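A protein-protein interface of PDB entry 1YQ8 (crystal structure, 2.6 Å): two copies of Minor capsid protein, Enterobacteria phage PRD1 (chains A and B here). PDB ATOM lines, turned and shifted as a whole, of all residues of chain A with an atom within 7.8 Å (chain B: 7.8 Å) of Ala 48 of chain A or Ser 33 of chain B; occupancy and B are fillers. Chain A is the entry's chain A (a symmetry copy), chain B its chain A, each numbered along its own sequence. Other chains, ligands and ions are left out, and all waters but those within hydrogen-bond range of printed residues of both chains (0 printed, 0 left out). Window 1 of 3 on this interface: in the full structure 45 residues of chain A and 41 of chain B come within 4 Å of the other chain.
The backbone carbonyl oxygen of Ser 30 of chain B lies within hydrogen-bond range of the backbone NH of Ile 46 of chain A, at 2.8 Å. The backbone NH of Gly 32 of chain B is in hydrogen-bond range of the backbone carbonyl oxygen of Ile 46 of chain A (2.6 Å). The side-chain hydroxyl (OG) of Ser 33 of chain B is in hydrogen-bond range of the side-chain carboxylate (OE1) of Glu 47 of chain A (3.5 Å). The backbone carbonyl oxygen (O) of Ser 33 of chain B is in hydrogen-bond range of the backbone NH (N) of Ala 48 of chain A (3.2 Å). The side-chain amide nitrogen (ND2) of Asn 191 of chain B sits close to the backbone NH (N) of Val 50 of chain A, 2.4 Å away.
O of Gly 34 of chain B sits at hydrogen-bond distance from N of Ser 49 of chain B. The side-chain amino group (NZ) of Lys 189 of chain B is in salt-bridge range of the chain-end carboxylate (O) of Asn 191 of chain B (2.9 Å). O of Gly 34 of chain A sits at hydrogen-bond distance from N of Ser 49 of chain A, 2.9 Å away. The backbone NH (N) of Thr 36 of chain A lies within hydrogen-bond range of the backbone carbonyl oxygen (O) of Glu 47 of chain A, at 2.7 Å.
Among the printed residues, merely in contact across the chains: Ile 35 of chain A with Ile 35 of chain B (3.97 Å), Glu 45 of chain A with Ser 30 of chain B (3.5 Å), Glu 45 of chain A with Gly 32 of chain B (3.8 Å), Ile 46 of chain A with Gly 31 of chain B (3.4 Å), Ile 46 of chain A with Ile 35 of chain B (3.5 Å), Glu 47 of chain A with Gly 32 of chain B (3.8 Å), Glu 47 of chain A with Ile 35 of chain B (3.97 Å), Ala 48 of chain A with Gly 34 of chain B (3.997 Å), Ala 48 of chain A with Ile 35 of chain B (3.6 Å), Ser 49 of chain A with Asn 191 of chain B (3.2 Å) and Val 50 of chain A with Ile 190 of chain B (3.8 Å).
Of the printed residues of chain B, Ile 35 of chain A touches Ile 35 (3.97 Å). Val 37 of chain A touches none of the printed residues of chain B. Printed residues of chain B within 4 Å of Ile 46 of chain A: Ser 30, Gly 31, Gly 32 and Ile 35. Of chain B, only Gly 32 (3.8 Å), Ser 33 (3.5 Å) and Ile 35 (3.97 Å) come within 4 Å of Glu 47 of chain A. Printed residues of chain B within 4 Å of Ala 48 of chain A: Ser 33 (3.0 Å), Gly 34 (3.997 Å) and Ile 35 (3.6 Å). Of chain A, only Glu 45 (3.8 Å), Ile 46 (2.6 Å) and Glu 47 (3.8 Å) come within 4 Å of Gly 32 of chain B. Ser 33 of chain B touches just these residues of chain A: Glu 47 (3.5 Å) and Ala 48 (3.0 Å). The nearest residue of chain A that does not touch Ser 33 of chain B is Ile 46 of chain A (4.9 Å).
Of the 12 printed residues of chain A, 7 touch a printed residue of chain B. Printed residues of chain A that touch a printed residue of chain B: Ile 35, Glu 45, Ile 46, Glu 47, Ala 48, Ser 49 and Val 50. Hydrophobic or aromatic side chains of chain A that line the printed part of chain B: Ile 35, Ile 46, Ala 48 and Val 50. Along chain A the printed residues that touch a printed residue of chain B span positions 35 to 50. Of the 18 printed residues of chain B, 8 touch a printed residue of chain A. Printed residues of chain B that touch a printed residue of chain A: Ser 30, Gly 31, Gly 32, Ser 33, Gly 34, Ile 35, Ile 190 and Asn 191. Hydrophobic or aromatic side chains of chain B within 4 Å of the printed part of chain A: Ile 35. Among the printed residues, 16 pairs touch across the chains. Among the printed residues, no Asp or Glu carboxylate lies within 4 Å of a Lys or Arg side-chain nitrogen of the other chain.
Ile 35 of chain B touches its own counterpart, Ile 35 of chain A. Glu 47 of chain A touches Ile 35 of chain B, but with the chains exchanged Ile 35 of chain A does not touch Glu 47 of chain B (7.2 Å). Ala 48 of chain A touches Ser 33 of chain B, but with the chains exchanged Ser 33 of chain A does not touch Ala 48 of chain B (8.8 Å). Ala 48 of chain A touches Gly 34 of chain B, but with the chains exchanged Gly 34 of chain A does not touch Ala 48 of chain B (7.3 Å). Positions printed for both chains: 33, 34, 35, 36, 47, 48, 49, 50 and 51.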
ATOM      1  N   SER A  33       4.756  27.358  31.501  1.00  0.00           N
ATOM      2  CA  SER A  33       4.113  27.386  30.189  1.00  0.00           C
ATOM      3  C   SER A  33       4.373  26.188  29.285  1.00  0.00           C
ATOM      4  O   SER A  33       5.460  26.044  28.718  1.00  0.00           O
ATOM      5  CB  SER A  33       4.518  28.658  29.439  1.00  0.00           C
ATOM      6  OG  SER A  33       4.032  29.805  30.117  1.00  0.00           O
ATOM      7  N   GLY A  34       3.354  25.350  29.128  1.00  0.00           N
ATOM      8  CA  GLY A  34       3.486  24.192  28.266  1.00  0.00           C
ATOM      9  C   GLY A  34       3.860  22.946  29.032  1.00  0.00           C
ATOM     10  O   GLY A  34       4.229  21.928  28.444  1.00  0.00           O
ATOM     11  N   ILE A  35       3.750  23.013  30.351  1.00  0.00           N
ATOM     12  CA  ILE A  35       4.102  21.879  31.174  1.00  0.00           C
ATOM     13  C   ILE A  35       3.033  21.557  32.208  1.00  0.00           C
ATOM     14  O   ILE A  35       2.249  22.417  32.621  1.00  0.00           O
ATOM     15  CB  ILE A  35       5.448  22.136  31.885  1.00  0.00           C
ATOM     16  CG1 ILE A  35       6.578  22.198  30.848  1.00  0.00           C
ATOM     17  CG2 ILE A  35       5.715  21.056  32.915  1.00  0.00           C
ATOM     18  CD1 ILE A  35       6.832  20.884  30.114  1.00  0.00           C
ATOM     19  N   THR A  36       3.003  20.293  32.604  1.00  0.00           N
ATOM     20  CA  THR A  36       2.076  19.814  33.607  1.00  0.00           C
ATOM     21  C   THR A  36       2.813  18.857  34.537  1.00  0.00           C
ATOM     22  O   THR A  36       3.416  17.881  34.097  1.00  0.00           O
ATOM     23  CB  THR A  36       0.875  19.078  32.966  1.00  0.00           C
ATOM     24  OG1 THR A  36      -0.077  20.034  32.494  1.00  0.00           O
ATOM     25  CG2 THR A  36       0.197  18.178  33.976  1.00  0.00           C
ATOM     26  N   VAL A  37       2.800  19.167  35.822  1.00  0.00           N
ATOM     27  CA  VAL A  37       3.416  18.300  36.798  1.00  0.00           C
ATOM     28  C   VAL A  37       2.222  17.691  37.528  1.00  0.00           C
ATOM     29  O   VAL A  37       1.505  18.369  38.272  1.00  0.00           O
ATOM     30  CB  VAL A  37       4.331  19.087  37.753  1.00  0.00           C
ATOM     31  CG1 VAL A  37       5.461  19.720  36.962  1.00  0.00           C
ATOM     32  CG2 VAL A  37       3.557  20.162  38.463  1.00  0.00           C
ATOM     33  N   GLU A  45       4.895  13.589  37.907  1.00  0.00           N
ATOM     34  CA  GLU A  45       5.084  13.441  36.465  1.00  0.00           C
ATOM     35  C   GLU A  45       5.141  14.756  35.705  1.00  0.00           C
ATOM     36  O   GLU A  45       4.211  15.564  35.765  1.00  0.00           O
ATOM     37  CB  GLU A  45       3.973  12.581  35.864  1.00  0.00           C
ATOM     38  CG  GLU A  45       4.239  12.173  34.424  1.00  0.00           C
ATOM     39  CD  GLU A  45       3.093  11.394  33.816  1.00  0.00           C
ATOM     40  OE1 GLU A  45       2.025  12.004  33.604  1.00  0.00           O
ATOM     41  OE2 GLU A  45       3.255  10.175  33.561  1.00  0.00           O
ATOM     42  N   ILE A  46       6.245  14.959  34.990  1.00  0.00           N
ATOM     43  CA  ILE A  46       6.428  16.152  34.181  1.00  0.00           C
ATOM     44  C   ILE A  46       5.961  15.807  32.763  1.00  0.00           C
ATOM     45  O   ILE A  46       6.549  14.970  32.069  1.00  0.00           O
ATOM     46  CB  ILE A  46       7.904  16.599  34.164  1.00  0.00           C
ATOM     47  CG1 ILE A  46       8.343  16.948  35.579  1.00  0.00           C
ATOM     48  CG2 ILE A  46       8.088  17.794  33.246  1.00  0.00           C
ATOM     49  CD1 ILE A  46       9.735  17.532  35.657  1.00  0.00           C
ATOM     50  N   GLU A  47       4.877  16.454  32.360  1.00  0.00           N
ATOM     51  CA  GLU A  47       4.280  16.240  31.048  1.00  0.00           C
ATOM     52  C   GLU A  47       4.304  17.571  30.297  1.00  0.00           C
ATOM     53  O   GLU A  47       4.238  18.640  30.912  1.00  0.00           O
ATOM     54  CB  GLU A  47       2.840  15.712  31.227  1.00  0.00           C
ATOM     55  CG  GLU A  47       2.061  15.436  29.951  1.00  0.00           C
ATOM     56  CD  GLU A  47       1.271  14.108  29.990  1.00  0.00           C
ATOM     57  OE1 GLU A  47       0.372  13.933  29.130  1.00  0.00           O
ATOM     58  OE2 GLU A  47       1.548  13.234  30.855  1.00  0.00           O
ATOM     59  N   ALA A  48       4.426  17.501  28.976  1.00  0.00           N
ATOM     60  CA  ALA A  48       4.468  18.696  28.144  1.00  0.00           C
ATOM     61  C   ALA A  48       3.294  18.743  27.181  1.00  0.00           C
ATOM     62  O   ALA A  48       2.721  17.712  26.815  1.00  0.00           O
ATOM     63  CB  ALA A  48       5.760  18.737  27.375  1.00  0.00           C
ATOM     64  N   SER A  49       2.938  19.952  26.776  1.00  0.00           N
ATOM     65  CA  SER A  49       1.839  20.172  25.846  1.00  0.00           C
ATOM     66  C   SER A  49       1.870  21.643  25.461  1.00  0.00           C
ATOM     67  O   SER A  49       2.681  22.394  25.986  1.00  0.00           O
ATOM     68  CB  SER A  49       0.507  19.824  26.510  1.00  0.00           C
ATOM     69  OG  SER A  49       0.310  20.579  27.689  1.00  0.00           O
ATOM     70  N   VAL A  50       1.014  22.064  24.539  1.00  0.00           N
ATOM     71  CA  VAL A  50       1.017  23.460  24.148  1.00  0.00           C
ATOM     72  C   VAL A  50       0.138  24.256  25.079  1.00  0.00           C
ATOM     73  O   VAL A  50      -0.760  23.726  25.724  1.00  0.00           O
ATOM     74  CB  VAL A  50       0.524  23.665  22.715  1.00  0.00           C
ATOM     75  CG1 VAL A  50       1.369  22.847  21.765  1.00  0.00           C
ATOM     76  CG2 VAL A  50      -0.952  23.307  22.610  1.00  0.00           C
ATOM     77  N   THR A  51       0.405  25.547  25.142  1.00  0.00           N
ATOM     78  CA  THR A  51      -0.348  26.430  26.010  1.00  0.00           C
ATOM     79  C   THR A  51      -1.766  26.647  25.520  1.00  0.00           C
ATOM     80  O   THR A  51      -2.728  26.451  26.268  1.00  0.00           O
ATOM     81  CB  THR A  51       0.355  27.791  26.134  1.00  0.00           C
ATOM     82  OG1 THR A  51       0.520  28.364  24.831  1.00  0.00           O
ATOM     83  CG2 THR A  51       1.712  27.616  26.781  1.00  0.00           C
ATOM     84  N   SER B  30       9.198  11.499  36.850  1.00  0.00           N
ATOM     85  CA  SER B  30       8.995  10.836  35.562  1.00  0.00           C
ATOM     86  C   SER B  30       8.641  11.823  34.453  1.00  0.00           C
ATOM     87  O   SER B  30       8.096  12.908  34.700  1.00  0.00           O
ATOM     88  CB  SER B  30       7.881   9.795  35.669  1.00  0.00           C
ATOM     89  OG  SER B  30       6.672  10.384  36.128  1.00  0.00           O
ATOM     90  N   GLY B  31       8.950  11.444  33.224  1.00  0.00           N
ATOM     91  CA  GLY B  31       8.637  12.308  32.109  1.00  0.00           C
ATOM     92  C   GLY B  31       7.468  11.744  31.331  1.00  0.00           C
ATOM     93  O   GLY B  31       7.558  10.647  30.777  1.00  0.00           O
ATOM     94  N   GLY B  32       6.367  12.492  31.294  1.00  0.00           N
ATOM     95  CA  GLY B  32       5.193  12.047  30.563  1.00  0.00           C
ATOM     96  C   GLY B  32       5.293  12.255  29.057  1.00  0.00           C
ATOM     97  O   GLY B  32       6.344  12.043  28.437  1.00  0.00           O
ATOM     98  N   SER B  33       4.187  12.692  28.466  1.00  0.00           N
ATOM     99  CA  SER B  33       4.108  12.919  27.025  1.00  0.00           C
ATOM    100  C   SER B  33       4.884  14.114  26.487  1.00  0.00           C
ATOM    101  O   SER B  33       4.476  15.267  26.662  1.00  0.00           O
ATOM    102  CB  SER B  33       2.644  13.057  26.600  1.00  0.00           C
ATOM    103  OG  SER B  33       1.949  11.841  26.824  1.00  0.00           O
ATOM    104  N   GLY B  34       5.986  13.828  25.801  1.00  0.00           N
ATOM    105  CA  GLY B  34       6.781  14.891  25.222  1.00  0.00           C
ATOM    106  C   GLY B  34       7.933  15.297  26.110  1.00  0.00           C
ATOM    107  O   GLY B  34       8.576  16.323  25.886  1.00  0.00           O
ATOM    108  N   ILE B  35       8.211  14.481  27.117  1.00  0.00           N
ATOM    109  CA  ILE B  35       9.282  14.790  28.036  1.00  0.00           C
ATOM    110  C   ILE B  35      10.207  13.604  28.270  1.00  0.00           C
ATOM    111  O   ILE B  35       9.823  12.441  28.118  1.00  0.00           O
ATOM    112  CB  ILE B  35       8.706  15.269  29.384  1.00  0.00           C
ATOM    113  CG1 ILE B  35       7.991  16.614  29.193  1.00  0.00           C
ATOM    114  CG2 ILE B  35       9.808  15.382  30.420  1.00  0.00           C
ATOM    115  CD1 ILE B  35       8.910  17.765  28.795  1.00  0.00           C
ATOM    116  N   THR B  36      11.444  13.924  28.625  1.00  0.00           N
ATOM    117  CA  THR B  36      12.449  12.926  28.921  1.00  0.00           C
ATOM    118  C   THR B  36      13.241  13.379  30.143  1.00  0.00           C
ATOM    119  O   THR B  36      13.792  14.476  30.173  1.00  0.00           O
ATOM    120  CB  THR B  36      13.420  12.723  27.732  1.00  0.00           C
ATOM    121  OG1 THR B  36      12.812  11.870  26.758  1.00  0.00           O
ATOM    122  CG2 THR B  36      14.710  12.085  28.197  1.00  0.00           C
ATOM    123  N   GLU B  47      14.133  17.086  29.662  1.00  0.00           N
ATOM    124  CA  GLU B  47      14.254  17.451  28.257  1.00  0.00           C
ATOM    125  C   GLU B  47      12.880  17.289  27.608  1.00  0.00           C
ATOM    126  O   GLU B  47      12.083  16.444  28.029  1.00  0.00           O
ATOM    127  CB  GLU B  47      15.312  16.546  27.588  1.00  0.00           C
ATOM    128  CG  GLU B  47      15.566  16.787  26.109  1.00  0.00           C
ATOM    129  CD  GLU B  47      17.065  16.775  25.735  1.00  0.00           C
ATOM    130  OE1 GLU B  47      17.368  16.664  24.520  1.00  0.00           O
ATOM    131  OE2 GLU B  47      17.941  16.895  26.634  1.00  0.00           O
ATOM    132  N   ALA B  48      12.600  18.116  26.606  1.00  0.00           N
ATOM    133  CA  ALA B  48      11.323  18.070  25.907  1.00  0.00           C
ATOM    134  C   ALA B  48      11.506  17.717  24.440  1.00  0.00           C
ATOM    135  O   ALA B  48      12.566  17.949  23.851  1.00  0.00           O
ATOM    136  CB  ALA B  48      10.626  19.396  26.029  1.00  0.00           C
ATOM    137  N   SER B  49      10.462  17.147  23.857  1.00  0.00           N
ATOM    138  CA  SER B  49      10.469  16.755  22.454  1.00  0.00           C
ATOM    139  C   SER B  49       9.048  16.342  22.102  1.00  0.00           C
ATOM    140  O   SER B  49       8.186  16.318  22.969  1.00  0.00           O
ATOM    141  CB  SER B  49      11.433  15.590  22.236  1.00  0.00           C
ATOM    142  OG  SER B  49      11.094  14.487  23.052  1.00  0.00           O
ATOM    143  N   VAL B  50       8.785  16.033  20.839  1.00  0.00           N
ATOM    144  CA  VAL B  50       7.442  15.634  20.467  1.00  0.00           C
ATOM    145  C   VAL B  50       7.268  14.153  20.684  1.00  0.00           C
ATOM    146  O   VAL B  50       8.227  13.390  20.709  1.00  0.00           O
ATOM    147  CB  VAL B  50       7.120  15.956  19.007  1.00  0.00           C
ATOM    148  CG1 VAL B  50       7.323  17.433  18.756  1.00  0.00           C
ATOM    149  CG2 VAL B  50       7.975  15.103  18.080  1.00  0.00           C
ATOM    150  N   THR B  51       6.021  13.748  20.840  1.00  0.00           N
ATOM    151  CA  THR B  51       5.707  12.353  21.075  1.00  0.00           C
ATOM    152  C   THR B  51       5.936  11.497  19.845  1.00  0.00           C
ATOM    153  O   THR B  51       6.642  10.486  19.905  1.00  0.00           O
ATOM    154  CB  THR B  51       4.246  12.199  21.531  1.00  0.00           C
ATOM    155  OG1 THR B  51       3.377  12.766  20.543  1.00  0.00           O
ATOM    156  CG2 THR B  51       4.039  12.909  22.850  1.00  0.00           C
ATOM    157  N   ASP B  52       5.352  11.910  18.728  1.00  0.00           N
ATOM    158  CA  ASP B  52       5.480  11.139  17.511  1.00  0.00           C
ATOM    159  C   ASP B  52       5.671  11.987  16.261  1.00  0.00           C
ATOM    160  O   ASP B  52       5.144  13.097  16.149  1.00  0.00           O
ATOM    161  CB  ASP B  52       4.251  10.245  17.366  1.00  0.00           C
ATOM    162  CG  ASP B  52       3.792   9.670  18.698  1.00  0.00           C
ATOM    163  OD1 ASP B  52       3.106  10.394  19.446  1.00  0.00           O
ATOM    164  OD2 ASP B  52       4.131   8.505  19.002  1.00  0.00           O
ATOM    165  N   GLY B 103      -5.177   5.929  21.485  1.00  0.00           N
ATOM    166  CA  GLY B 103      -4.909   7.027  22.396  1.00  0.00           C
ATOM    167  C   GLY B 103      -3.984   8.090  21.846  1.00  0.00           C
ATOM    168  O   GLY B 103      -3.339   8.802  22.605  1.00  0.00           O
ATOM    169  N   LYS B 104      -3.917   8.217  20.530  1.00  0.00           N
ATOM    170  CA  LYS B 104      -3.031   9.205  19.924  1.00  0.00           C
ATOM    171  C   LYS B 104      -3.769  10.405  19.355  1.00  0.00           C
ATOM    172  O   LYS B 104      -3.200  11.169  18.561  1.00  0.00           O
ATOM    173  CB  LYS B 104      -2.181   8.552  18.828  1.00  0.00           C
ATOM    174  CG  LYS B 104      -0.927   7.886  19.344  1.00  0.00           C
ATOM    175  CD  LYS B 104      -0.033   8.907  19.985  1.00  0.00           C
ATOM    176  CE  LYS B 104       1.117   8.256  20.705  1.00  0.00           C
ATOM    177  NZ  LYS B 104       1.922   9.249  21.470  1.00  0.00           N
ATOM    178  N   LYS B 189       2.926  15.029  15.566  1.00  0.00           N
ATOM    179  CA  LYS B 189       1.912  15.303  16.567  1.00  0.00           C
ATOM    180  C   LYS B 189       2.499  16.321  17.536  1.00  0.00           C
ATOM    181  O   LYS B 189       3.497  16.047  18.197  1.00  0.00           O
ATOM    182  CB  LYS B 189       1.538  14.033  17.328  1.00  0.00           C
ATOM    183  CG  LYS B 189       0.659  14.323  18.533  1.00  0.00           C
ATOM    184  CD  LYS B 189       0.034  13.077  19.113  1.00  0.00           C
ATOM    185  CE  LYS B 189      -0.794  13.416  20.338  1.00  0.00           C
ATOM    186  NZ  LYS B 189       0.055  13.990  21.419  1.00  0.00           N
ATOM    187  N   ILE B 190       1.891  17.497  17.639  1.00  0.00           N
ATOM    188  CA  ILE B 190       2.439  18.489  18.551  1.00  0.00           C
ATOM    189  C   ILE B 190       1.702  18.608  19.898  1.00  0.00           C
ATOM    190  O   ILE B 190       2.193  19.269  20.818  1.00  0.00           O
ATOM    191  CB  ILE B 190       2.557  19.870  17.849  1.00  0.00           C
ATOM    192  CG1 ILE B 190       1.179  20.429  17.496  1.00  0.00           C
ATOM    193  CG2 ILE B 190       3.368  19.720  16.569  1.00  0.00           C
ATOM    194  CD1 ILE B 190       1.238  21.803  16.825  1.00  0.00           C
ATOM    195  N   ASN B 191       0.554  17.941  20.028  1.00  0.00           N
ATOM    196  CA  ASN B 191      -0.220  17.981  21.273  1.00  0.00           C
ATOM    197  C   ASN B 191      -1.339  16.937  21.302  1.00  0.00           C
ATOM    198  O   ASN B 191      -1.521  16.277  22.354  1.00  0.00           O
ATOM    199  CB  ASN B 191      -0.822  19.373  21.479  1.00  0.00           C
ATOM    200  CG  ASN B 191      -1.303  19.606  22.914  1.00  0.00           C
ATOM    201  OD1 ASN B 191      -2.238  18.963  23.387  1.00  0.00           O
ATOM    202  ND2 ASN B 191      -0.658  20.537  23.607  1.00  0.00           N
ATOM    203  OXT ASN B 191      -2.036  16.796  20.271  1.00  0.00           O
